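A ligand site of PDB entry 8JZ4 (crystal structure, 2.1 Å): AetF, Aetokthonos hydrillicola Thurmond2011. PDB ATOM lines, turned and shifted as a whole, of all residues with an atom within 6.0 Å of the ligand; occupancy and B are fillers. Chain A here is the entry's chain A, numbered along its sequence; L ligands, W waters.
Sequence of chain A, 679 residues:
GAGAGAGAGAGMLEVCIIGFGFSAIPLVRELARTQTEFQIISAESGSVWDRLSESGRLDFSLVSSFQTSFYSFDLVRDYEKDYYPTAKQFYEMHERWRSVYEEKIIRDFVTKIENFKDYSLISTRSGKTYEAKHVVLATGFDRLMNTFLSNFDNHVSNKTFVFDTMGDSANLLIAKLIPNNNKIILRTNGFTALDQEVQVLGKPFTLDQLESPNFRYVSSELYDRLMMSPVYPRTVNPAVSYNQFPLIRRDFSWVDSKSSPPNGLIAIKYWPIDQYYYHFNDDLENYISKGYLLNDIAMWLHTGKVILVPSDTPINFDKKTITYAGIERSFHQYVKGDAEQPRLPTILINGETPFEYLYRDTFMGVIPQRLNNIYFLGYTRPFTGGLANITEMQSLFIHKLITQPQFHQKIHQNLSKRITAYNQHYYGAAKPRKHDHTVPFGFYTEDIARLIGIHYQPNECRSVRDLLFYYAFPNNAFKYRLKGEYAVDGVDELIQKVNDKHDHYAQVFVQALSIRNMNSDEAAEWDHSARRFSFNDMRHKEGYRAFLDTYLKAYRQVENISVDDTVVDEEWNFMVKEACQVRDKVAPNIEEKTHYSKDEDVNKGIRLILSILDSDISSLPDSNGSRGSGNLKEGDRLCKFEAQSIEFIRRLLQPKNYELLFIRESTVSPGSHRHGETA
The side-chain hydroxyl of Ser 534 lies within hydrogen-bond range of an oxygen (O2) of the ligand (2.9 Å).
O of Leu 226 sits at hydrogen-bond distance from N1 of the ligand (2.9 Å).
N1 of the ligand is in hydrogen-bond range of OE1 of Gln 511 (2.8 Å).
The backbone carbonyl oxygen (O) of Leu 207 is in hydrogen-bond range of a nitrogen (N2) of the ligand (3.1 Å).
The side-chain amino group of Lys 598 lies within salt-bridge range of an oxygen (O2) of the ligand (3.4 Å).
The side-chain carboxylate (OD2) of Asp 527 is in salt-bridge range of a nitrogen (N1) of the ligand.
The side-chain hydroxyl of Thr 384 sits at hydrogen-bond distance from the side-chain carboxylate of Glu 211 (2.5 Å).
The side-chain amide nitrogen (NE2) of Gln 511 sits close to the side-chain amide nitrogen (NE2) of Gln 507 (2.9 Å).
OD1 of Asp 527 is in salt-bridge range of NZ of Lys 598 (2.7 Å).
The side-chain amino group (NZ) of Lys 598 sits at hydrogen-bond distance from the side-chain amide oxygen (OE1) of Gln 511.
Merely in contact with the ligand: Leu 210, Glu 211, Met 227, Val 231, Phe 535 and Phe 383.
Hydrophobic or aromatic side chains within 4 Å of the ligand: Leu 210, Leu 226, Met 227, Val 231, Phe 383 and Phe 535.
12 residues have an atom within 4 Å of the ligand: Leu 207, Leu 210, Glu 211, Leu 226, Met 227, Val 231, Phe 383, Gln 511, Asp 527, Ser 534, Phe 535 and Lys 598.
Water W1 bridges O2 of the ligand and OD2 of Asp 527.
Water W2 lies within hydrogen-bond range of an oxygen (O1) of the ligand (2.9 Å), the side-chain amide oxygen of Gln 507 (3.0 Å), the side-chain amino group of Lys 598 (3.0 Å), the side-chain amide nitrogen of Gln 511 (3.1 Å) and the side-chain hydroxyl of Ser 534 (3.4 Å).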
ATOM      1  N   LEU A 194       0.539  33.581   2.161  1.00  0.00           N
ATOM      2  CA  LEU A 194      -0.076  32.859   3.303  1.00  0.00           C
ATOM      3  C   LEU A 194       1.006  32.538   4.340  1.00  0.00           C
ATOM      4  O   LEU A 194       2.087  31.998   3.974  1.00  0.00           O
ATOM      5  CB  LEU A 194      -0.754  31.575   2.805  1.00  0.00           C
ATOM      6  CG  LEU A 194      -1.840  31.746   1.742  1.00  0.00           C
ATOM      7  CD1 LEU A 194      -2.116  30.431   1.042  1.00  0.00           C
ATOM      8  CD2 LEU A 194      -3.126  32.283   2.341  1.00  0.00           C
ATOM      9  N   VAL A 198       0.344  28.477  11.505  1.00  0.00           N
ATOM     10  CA  VAL A 198      -0.839  29.018  12.233  1.00  0.00           C
ATOM     11  C   VAL A 198      -0.816  28.456  13.653  1.00  0.00           C
ATOM     12  O   VAL A 198      -0.619  27.227  13.804  1.00  0.00           O
ATOM     13  CB  VAL A 198      -2.127  28.623  11.494  1.00  0.00           C
ATOM     14  CG1 VAL A 198      -3.368  28.933  12.301  1.00  0.00           C
ATOM     15  CG2 VAL A 198      -2.198  29.275  10.131  1.00  0.00           C
ATOM     16  N   LEU A 207       0.293  25.365   7.449  1.00  0.00           N
ATOM     17  CA  LEU A 207      -1.010  25.630   6.760  1.00  0.00           C
ATOM     18  C   LEU A 207      -1.531  24.370   6.039  1.00  0.00           C
ATOM     19  O   LEU A 207      -2.751  24.192   6.053  1.00  0.00           O
ATOM     20  CB  LEU A 207      -0.916  26.876   5.848  1.00  0.00           C
ATOM     21  CG  LEU A 207      -0.304  26.725   4.452  1.00  0.00           C
ATOM     22  CD1 LEU A 207      -0.474  28.022   3.667  1.00  0.00           C
ATOM     23  CD2 LEU A 207       1.156  26.346   4.524  1.00  0.00           C
ATOM     24  N   ASP A 208      -0.649  23.497   5.556  1.00  0.00           N
ATOM     25  CA  ASP A 208      -0.955  22.234   4.808  1.00  0.00           C
ATOM     26  C   ASP A 208      -1.728  21.242   5.688  1.00  0.00           C
ATOM     27  O   ASP A 208      -2.491  20.412   5.123  1.00  0.00           O
ATOM     28  CB  ASP A 208       0.321  21.607   4.247  1.00  0.00           C
ATOM     29  CG  ASP A 208       1.365  21.396   5.322  1.00  0.00           C
ATOM     30  OD1 ASP A 208       1.940  22.422   5.786  1.00  0.00           O
ATOM     31  OD2 ASP A 208       1.555  20.229   5.740  1.00  0.00           O
ATOM     32  N   LEU A 210      -4.121  22.017   7.718  1.00  0.00           N
ATOM     33  CA  LEU A 210      -5.438  22.623   8.046  1.00  0.00           C
ATOM     34  C   LEU A 210      -6.364  22.706   6.815  1.00  0.00           C
ATOM     35  O   LEU A 210      -7.324  23.523   6.867  1.00  0.00           O
ATOM     36  CB  LEU A 210      -5.169  24.011   8.632  1.00  0.00           C
ATOM     37  CG  LEU A 210      -4.402  24.028   9.943  1.00  0.00           C
ATOM     38  CD1 LEU A 210      -4.254  25.431  10.481  1.00  0.00           C
ATOM     39  CD2 LEU A 210      -5.083  23.150  10.983  1.00  0.00           C
ATOM     40  N   GLU A 211      -6.148  21.882   5.788  1.00  0.00           N
ATOM     41  CA  GLU A 211      -6.864  22.004   4.473  1.00  0.00           C
ATOM     42  C   GLU A 211      -7.931  20.917   4.321  1.00  0.00           C
ATOM     43  O   GLU A 211      -8.744  21.049   3.404  1.00  0.00           O
ATOM     44  CB  GLU A 211      -5.856  21.939   3.320  1.00  0.00           C
ATOM     45  CG  GLU A 211      -4.776  23.028   3.377  1.00  0.00           C
ATOM     46  CD  GLU A 211      -3.776  23.043   2.222  1.00  0.00           C
ATOM     47  OE1 GLU A 211      -4.027  22.387   1.201  1.00  0.00           O
ATOM     48  OE2 GLU A 211      -2.725  23.711   2.335  1.00  0.00           O
ATOM     49  N   LEU A 226     -14.958  27.325   3.193  1.00  0.00           N
ATOM     50  CA  LEU A 226     -13.993  26.925   4.258  1.00  0.00           C
ATOM     51  C   LEU A 226     -12.584  27.410   3.909  1.00  0.00           C
ATOM     52  O   LEU A 226     -11.804  27.668   4.851  1.00  0.00           O
ATOM     53  CB  LEU A 226     -14.021  25.401   4.393  1.00  0.00           C
ATOM     54  CG  LEU A 226     -12.931  24.735   5.235  1.00  0.00           C
ATOM     55  CD1 LEU A 226     -12.923  25.273   6.669  1.00  0.00           C
ATOM     56  CD2 LEU A 226     -13.120  23.238   5.245  1.00  0.00           C
ATOM     57  N   MET A 227     -12.245  27.501   2.627  1.00  0.00           N
ATOM     58  CA  MET A 227     -10.811  27.647   2.205  1.00  0.00           C
ATOM     59  C   MET A 227     -10.509  29.057   1.691  1.00  0.00           C
ATOM     60  O   MET A 227      -9.399  29.520   1.940  1.00  0.00           O
ATOM     61  CB  MET A 227     -10.416  26.610   1.140  1.00  0.00           C
ATOM     62  CG  MET A 227     -10.290  25.182   1.644  1.00  0.00           C
ATOM     63  SD  MET A 227      -9.119  25.020   3.029  1.00  0.00           S
ATOM     64  CE  MET A 227      -7.569  24.977   2.136  1.00  0.00           C
ATOM     65  N   MET A 228     -11.411  29.696   0.964  1.00  0.00           N
ATOM     66  CA  MET A 228     -11.053  30.758   0.001  1.00  0.00           C
ATOM     67  C   MET A 228     -11.079  32.182   0.576  1.00  0.00           C
ATOM     68  O   MET A 228     -10.492  33.022  -0.098  1.00  0.00           O
ATOM     69  CB  MET A 228     -11.938  30.661  -1.235  1.00  0.00           C
ATOM     70  CG  MET A 228     -11.690  29.399  -2.042  1.00  0.00           C
ATOM     71  SD  MET A 228      -9.958  28.988  -2.428  1.00  0.00           S
ATOM     72  CE  MET A 228      -9.552  30.257  -3.630  1.00  0.00           C
ATOM     73  N   PRO A 230      -9.248  33.786   2.728  1.00  0.00           N
ATOM     74  CA  PRO A 230      -7.934  34.431   2.781  1.00  0.00           C
ATOM     75  C   PRO A 230      -7.374  34.831   1.414  1.00  0.00           C
ATOM     76  O   PRO A 230      -6.420  35.624   1.392  1.00  0.00           O
ATOM     77  CB  PRO A 230      -7.012  33.403   3.466  1.00  0.00           C
ATOM     78  CG  PRO A 230      -7.931  32.285   3.935  1.00  0.00           C
ATOM     79  CD  PRO A 230      -9.179  32.364   3.080  1.00  0.00           C
ATOM     80  N   VAL A 231      -7.980  34.333   0.331  1.00  0.00           N
ATOM     81  CA  VAL A 231      -7.489  34.426  -1.076  1.00  0.00           C
ATOM     82  C   VAL A 231      -8.352  35.445  -1.833  1.00  0.00           C
ATOM     83  O   VAL A 231      -7.786  36.381  -2.392  1.00  0.00           O
ATOM     84  CB  VAL A 231      -7.484  33.056  -1.783  1.00  0.00           C
ATOM     85  CG1 VAL A 231      -7.086  33.181  -3.247  1.00  0.00           C
ATOM     86  CG2 VAL A 231      -6.594  32.038  -1.080  1.00  0.00           C
ATOM     87  N   PRO A 261      -9.445  25.173  -3.690  1.00  0.00           N
ATOM     88  CA  PRO A 261      -8.805  26.206  -4.502  1.00  0.00           C
ATOM     89  C   PRO A 261      -8.481  25.701  -5.904  1.00  0.00           C
ATOM     90  O   PRO A 261      -8.240  24.522  -6.109  1.00  0.00           O
ATOM     91  CB  PRO A 261      -7.491  26.550  -3.773  1.00  0.00           C
ATOM     92  CG  PRO A 261      -7.313  25.475  -2.722  1.00  0.00           C
ATOM     93  CD  PRO A 261      -8.649  24.784  -2.531  1.00  0.00           C
ATOM     94  N   LEU A 265      -3.666  28.310  -9.206  1.00  0.00           N
ATOM     95  CA  LEU A 265      -3.467  29.305  -8.126  1.00  0.00           C
ATOM     96  C   LEU A 265      -2.115  29.061  -7.490  1.00  0.00           C
ATOM     97  O   LEU A 265      -1.845  27.883  -7.078  1.00  0.00           O
ATOM     98  CB  LEU A 265      -4.577  29.165  -7.073  1.00  0.00           C
ATOM     99  CG  LEU A 265      -4.551  30.243  -5.999  1.00  0.00           C
ATOM    100  CD1 LEU A 265      -5.105  31.541  -6.550  1.00  0.00           C
ATOM    101  CD2 LEU A 265      -5.335  29.801  -4.767  1.00  0.00           C
ATOM    102  N   PHE A 383       0.299  23.405  -4.501  1.00  0.00           N
ATOM    103  CA  PHE A 383      -0.172  24.753  -4.094  1.00  0.00           C
ATOM    104  C   PHE A 383       0.410  25.102  -2.724  1.00  0.00           C
ATOM    105  O   PHE A 383       0.869  26.237  -2.494  1.00  0.00           O
ATOM    106  CB  PHE A 383      -1.700  24.813  -4.162  1.00  0.00           C
ATOM    107  CG  PHE A 383      -2.302  26.068  -3.565  1.00  0.00           C
ATOM    108  CD1 PHE A 383      -1.913  27.324  -4.016  1.00  0.00           C
ATOM    109  CD2 PHE A 383      -3.269  25.976  -2.573  1.00  0.00           C
ATOM    110  CE1 PHE A 383      -2.473  28.469  -3.467  1.00  0.00           C
ATOM    111  CE2 PHE A 383      -3.828  27.121  -2.024  1.00  0.00           C
ATOM    112  CZ  PHE A 383      -3.421  28.357  -2.467  1.00  0.00           C
ATOM    113  N   THR A 384       0.464  24.114  -1.822  1.00  0.00           N
ATOM    114  CA  THR A 384       1.060  24.273  -0.472  1.00  0.00           C
ATOM    115  C   THR A 384       1.802  22.998  -0.116  1.00  0.00           C
ATOM    116  O   THR A 384       1.616  21.981  -0.799  1.00  0.00           O
ATOM    117  CB  THR A 384      -0.006  24.572   0.590  1.00  0.00           C
ATOM    118  OG1 THR A 384      -0.877  23.436   0.647  1.00  0.00           O
ATOM    119  CG2 THR A 384      -0.770  25.845   0.324  1.00  0.00           C
ATOM    120  N   GLN A 507      -9.490  19.813  15.279  1.00  0.00           N
ATOM    121  CA  GLN A 507      -9.732  21.265  15.053  1.00  0.00           C
ATOM    122  C   GLN A 507     -10.213  21.467  13.610  1.00  0.00           C
ATOM    123  O   GLN A 507     -11.244  22.132  13.434  1.00  0.00           O
ATOM    124  CB  GLN A 507      -8.498  22.136  15.306  1.00  0.00           C
ATOM    125  CG  GLN A 507      -8.802  23.635  15.207  1.00  0.00           C
ATOM    126  CD  GLN A 507      -8.617  24.341  13.872  1.00  0.00           C
ATOM    127  OE1 GLN A 507      -8.643  25.575  13.783  1.00  0.00           O
ATOM    128  NE2 GLN A 507      -8.467  23.590  12.802  1.00  0.00           N
ATOM    129  N   VAL A 508      -9.495  20.953  12.605  1.00  0.00           N
ATOM    130  CA  VAL A 508      -9.904  21.252  11.201  1.00  0.00           C
ATOM    131  C   VAL A 508     -11.246  20.554  10.931  1.00  0.00           C
ATOM    132  O   VAL A 508     -12.032  21.160  10.238  1.00  0.00           O
ATOM    133  CB  VAL A 508      -8.851  20.934  10.121  1.00  0.00           C
ATOM    134  CG1 VAL A 508      -8.566  19.453   9.943  1.00  0.00           C
ATOM    135  CG2 VAL A 508      -9.285  21.551   8.788  1.00  0.00           C
ATOM    136  N   GLN A 511     -13.822  22.880  12.085  1.00  0.00           N
ATOM    137  CA  GLN A 511     -13.909  24.058  11.194  1.00  0.00           C
ATOM    138  C   GLN A 511     -14.958  23.789  10.118  1.00  0.00           C
ATOM    139  O   GLN A 511     -15.824  24.600   9.959  1.00  0.00           O
ATOM    140  CB  GLN A 511     -12.571  24.392  10.549  1.00  0.00           C
ATOM    141  CG  GLN A 511     -11.646  25.241  11.396  1.00  0.00           C
ATOM    142  CD  GLN A 511     -10.536  25.825  10.553  1.00  0.00           C
ATOM    143  OE1 GLN A 511     -10.753  26.733   9.770  1.00  0.00           O
ATOM    144  NE2 GLN A 511      -9.347  25.289  10.688  1.00  0.00           N
ATOM    145  N   TRP A 526     -16.662  34.687   9.778  1.00  0.00           N
ATOM    146  CA  TRP A 526     -16.415  33.691  10.831  1.00  0.00           C
ATOM    147  C   TRP A 526     -14.909  33.351  10.882  1.00  0.00           C
ATOM    148  O   TRP A 526     -14.336  33.308  11.994  1.00  0.00           O
ATOM    149  CB  TRP A 526     -17.266  32.444  10.572  1.00  0.00           C
ATOM    150  CG  TRP A 526     -17.047  31.369  11.587  1.00  0.00           C
ATOM    151  CD1 TRP A 526     -17.723  31.207  12.755  1.00  0.00           C
ATOM    152  CD2 TRP A 526     -16.074  30.312  11.537  1.00  0.00           C
ATOM    153  NE1 TRP A 526     -17.246  30.118  13.430  1.00  0.00           N
ATOM    154  CE2 TRP A 526     -16.224  29.550  12.709  1.00  0.00           C
ATOM    155  CE3 TRP A 526     -15.071  29.950  10.621  1.00  0.00           C
ATOM    156  CZ2 TRP A 526     -15.412  28.455  13.003  1.00  0.00           C
ATOM    157  CZ3 TRP A 526     -14.277  28.856  10.906  1.00  0.00           C
ATOM    158  CH2 TRP A 526     -14.440  28.134  12.084  1.00  0.00           C
ATOM    159  N   ASP A 527     -14.303  33.114   9.716  1.00  0.00           N
ATOM    160  CA  ASP A 527     -12.865  32.720   9.609  1.00  0.00           C
ATOM    161  C   ASP A 527     -12.020  33.869  10.165  1.00  0.00           C
ATOM    162  O   ASP A 527     -10.973  33.581  10.782  1.00  0.00           O
ATOM    163  CB  ASP A 527     -12.495  32.295   8.186  1.00  0.00           C
ATOM    164  CG  ASP A 527     -11.674  31.013   8.045  1.00  0.00           C
ATOM    165  OD1 ASP A 527     -11.390  30.328   9.067  1.00  0.00           O
ATOM    166  OD2 ASP A 527     -11.301  30.710   6.895  1.00  0.00           O
ATOM    167  N   SER A 534      -5.804  33.037  10.711  1.00  0.00           N
ATOM    168  CA  SER A 534      -4.698  32.171  10.205  1.00  0.00           C
ATOM    169  C   SER A 534      -3.731  33.009   9.352  1.00  0.00           C
ATOM    170  O   SER A 534      -2.507  32.920   9.558  1.00  0.00           O
ATOM    171  CB  SER A 534      -5.280  30.983   9.455  1.00  0.00           C
ATOM    172  OG  SER A 534      -6.095  30.173  10.296  1.00  0.00           O
ATOM    173  N   PHE A 535      -4.254  33.826   8.437  1.00  0.00           N
ATOM    174  CA  PHE A 535      -3.440  34.433   7.358  1.00  0.00           C
ATOM    175  C   PHE A 535      -3.532  35.965   7.376  1.00  0.00           C
ATOM    176  O   PHE A 535      -4.644  36.553   7.471  1.00  0.00           O
ATOM    177  CB  PHE A 535      -3.869  33.820   6.025  1.00  0.00           C
ATOM    178  CG  PHE A 535      -3.808  32.318   6.025  1.00  0.00           C
ATOM    179  CD1 PHE A 535      -2.594  31.650   6.170  1.00  0.00           C
ATOM    180  CD2 PHE A 535      -4.971  31.572   5.911  1.00  0.00           C
ATOM    181  CE1 PHE A 535      -2.566  30.268   6.201  1.00  0.00           C
ATOM    182  CE2 PHE A 535      -4.926  30.180   5.928  1.00  0.00           C
ATOM    183  CZ  PHE A 535      -3.721  29.533   6.069  1.00  0.00           C
ATOM    184  N   LYS A 598     -15.002  32.219  16.088  1.00  0.00           N
ATOM    185  CA  LYS A 598     -14.183  31.067  15.646  1.00  0.00           C
ATOM    186  C   LYS A 598     -13.477  30.447  16.858  1.00  0.00           C
ATOM    187  O   LYS A 598     -13.522  29.204  16.978  1.00  0.00           O
ATOM    188  CB  LYS A 598     -13.175  31.470  14.570  1.00  0.00           C
ATOM    189  CG  LYS A 598     -12.222  30.363  14.174  1.00  0.00           C
ATOM    190  CD  LYS A 598     -11.680  30.484  12.781  1.00  0.00           C
ATOM    191  CE  LYS A 598     -10.645  29.413  12.493  1.00  0.00           C
ATOM    192  NZ  LYS A 598      -9.927  29.687  11.225  1.00  0.00           N
HETATM  193  O1  LIG L   1      -7.510  27.076   9.003  1.00  0.00           O
HETATM  194  C1  LIG L   1      -8.081  27.919   8.254  1.00  0.00           C
HETATM  195  O2  LIG L   1      -8.125  29.155   8.447  1.00  0.00           O
HETATM  196  C2  LIG L   1      -8.875  27.428   7.055  1.00  0.00           C
HETATM  197  N1  LIG L   1     -10.293  27.889   7.262  1.00  0.00           N
HETATM  198  C3  LIG L   1      -8.272  27.996   5.747  1.00  0.00           C
HETATM  199  C4  LIG L   1      -6.948  27.302   5.376  1.00  0.00           C
HETATM  200  C5  LIG L   1      -6.304  27.394   4.201  1.00  0.00           C
HETATM  201  C6  LIG L   1      -6.575  28.053   3.062  1.00  0.00           C
HETATM  202  C7  LIG L   1      -5.693  27.989   1.981  1.00  0.00           C
HETATM  203 BR1  LIG L   1      -6.142  28.976   0.324  1.00  0.00          BR
HETATM  204  C8  LIG L   1      -4.535  27.193   2.095  1.00  0.00           C
HETATM  205  C9  LIG L   1      -4.287  26.514   3.278  1.00  0.00           C
HETATM  206  C10 LIG L   1      -5.191  26.641   4.294  1.00  0.00           C
HETATM  207  N2  LIG L   1      -5.190  26.104   5.513  1.00  0.00           N
HETATM  208  C11 LIG L   1      -6.250  26.495   6.188  1.00  0.00           C
HETATM  209  O   HOH W   1      -8.543  31.317   7.299  1.00  0.00           O
HETATM  210  O   HOH W   2      -7.785  27.648  11.838  1.00  0.00           O
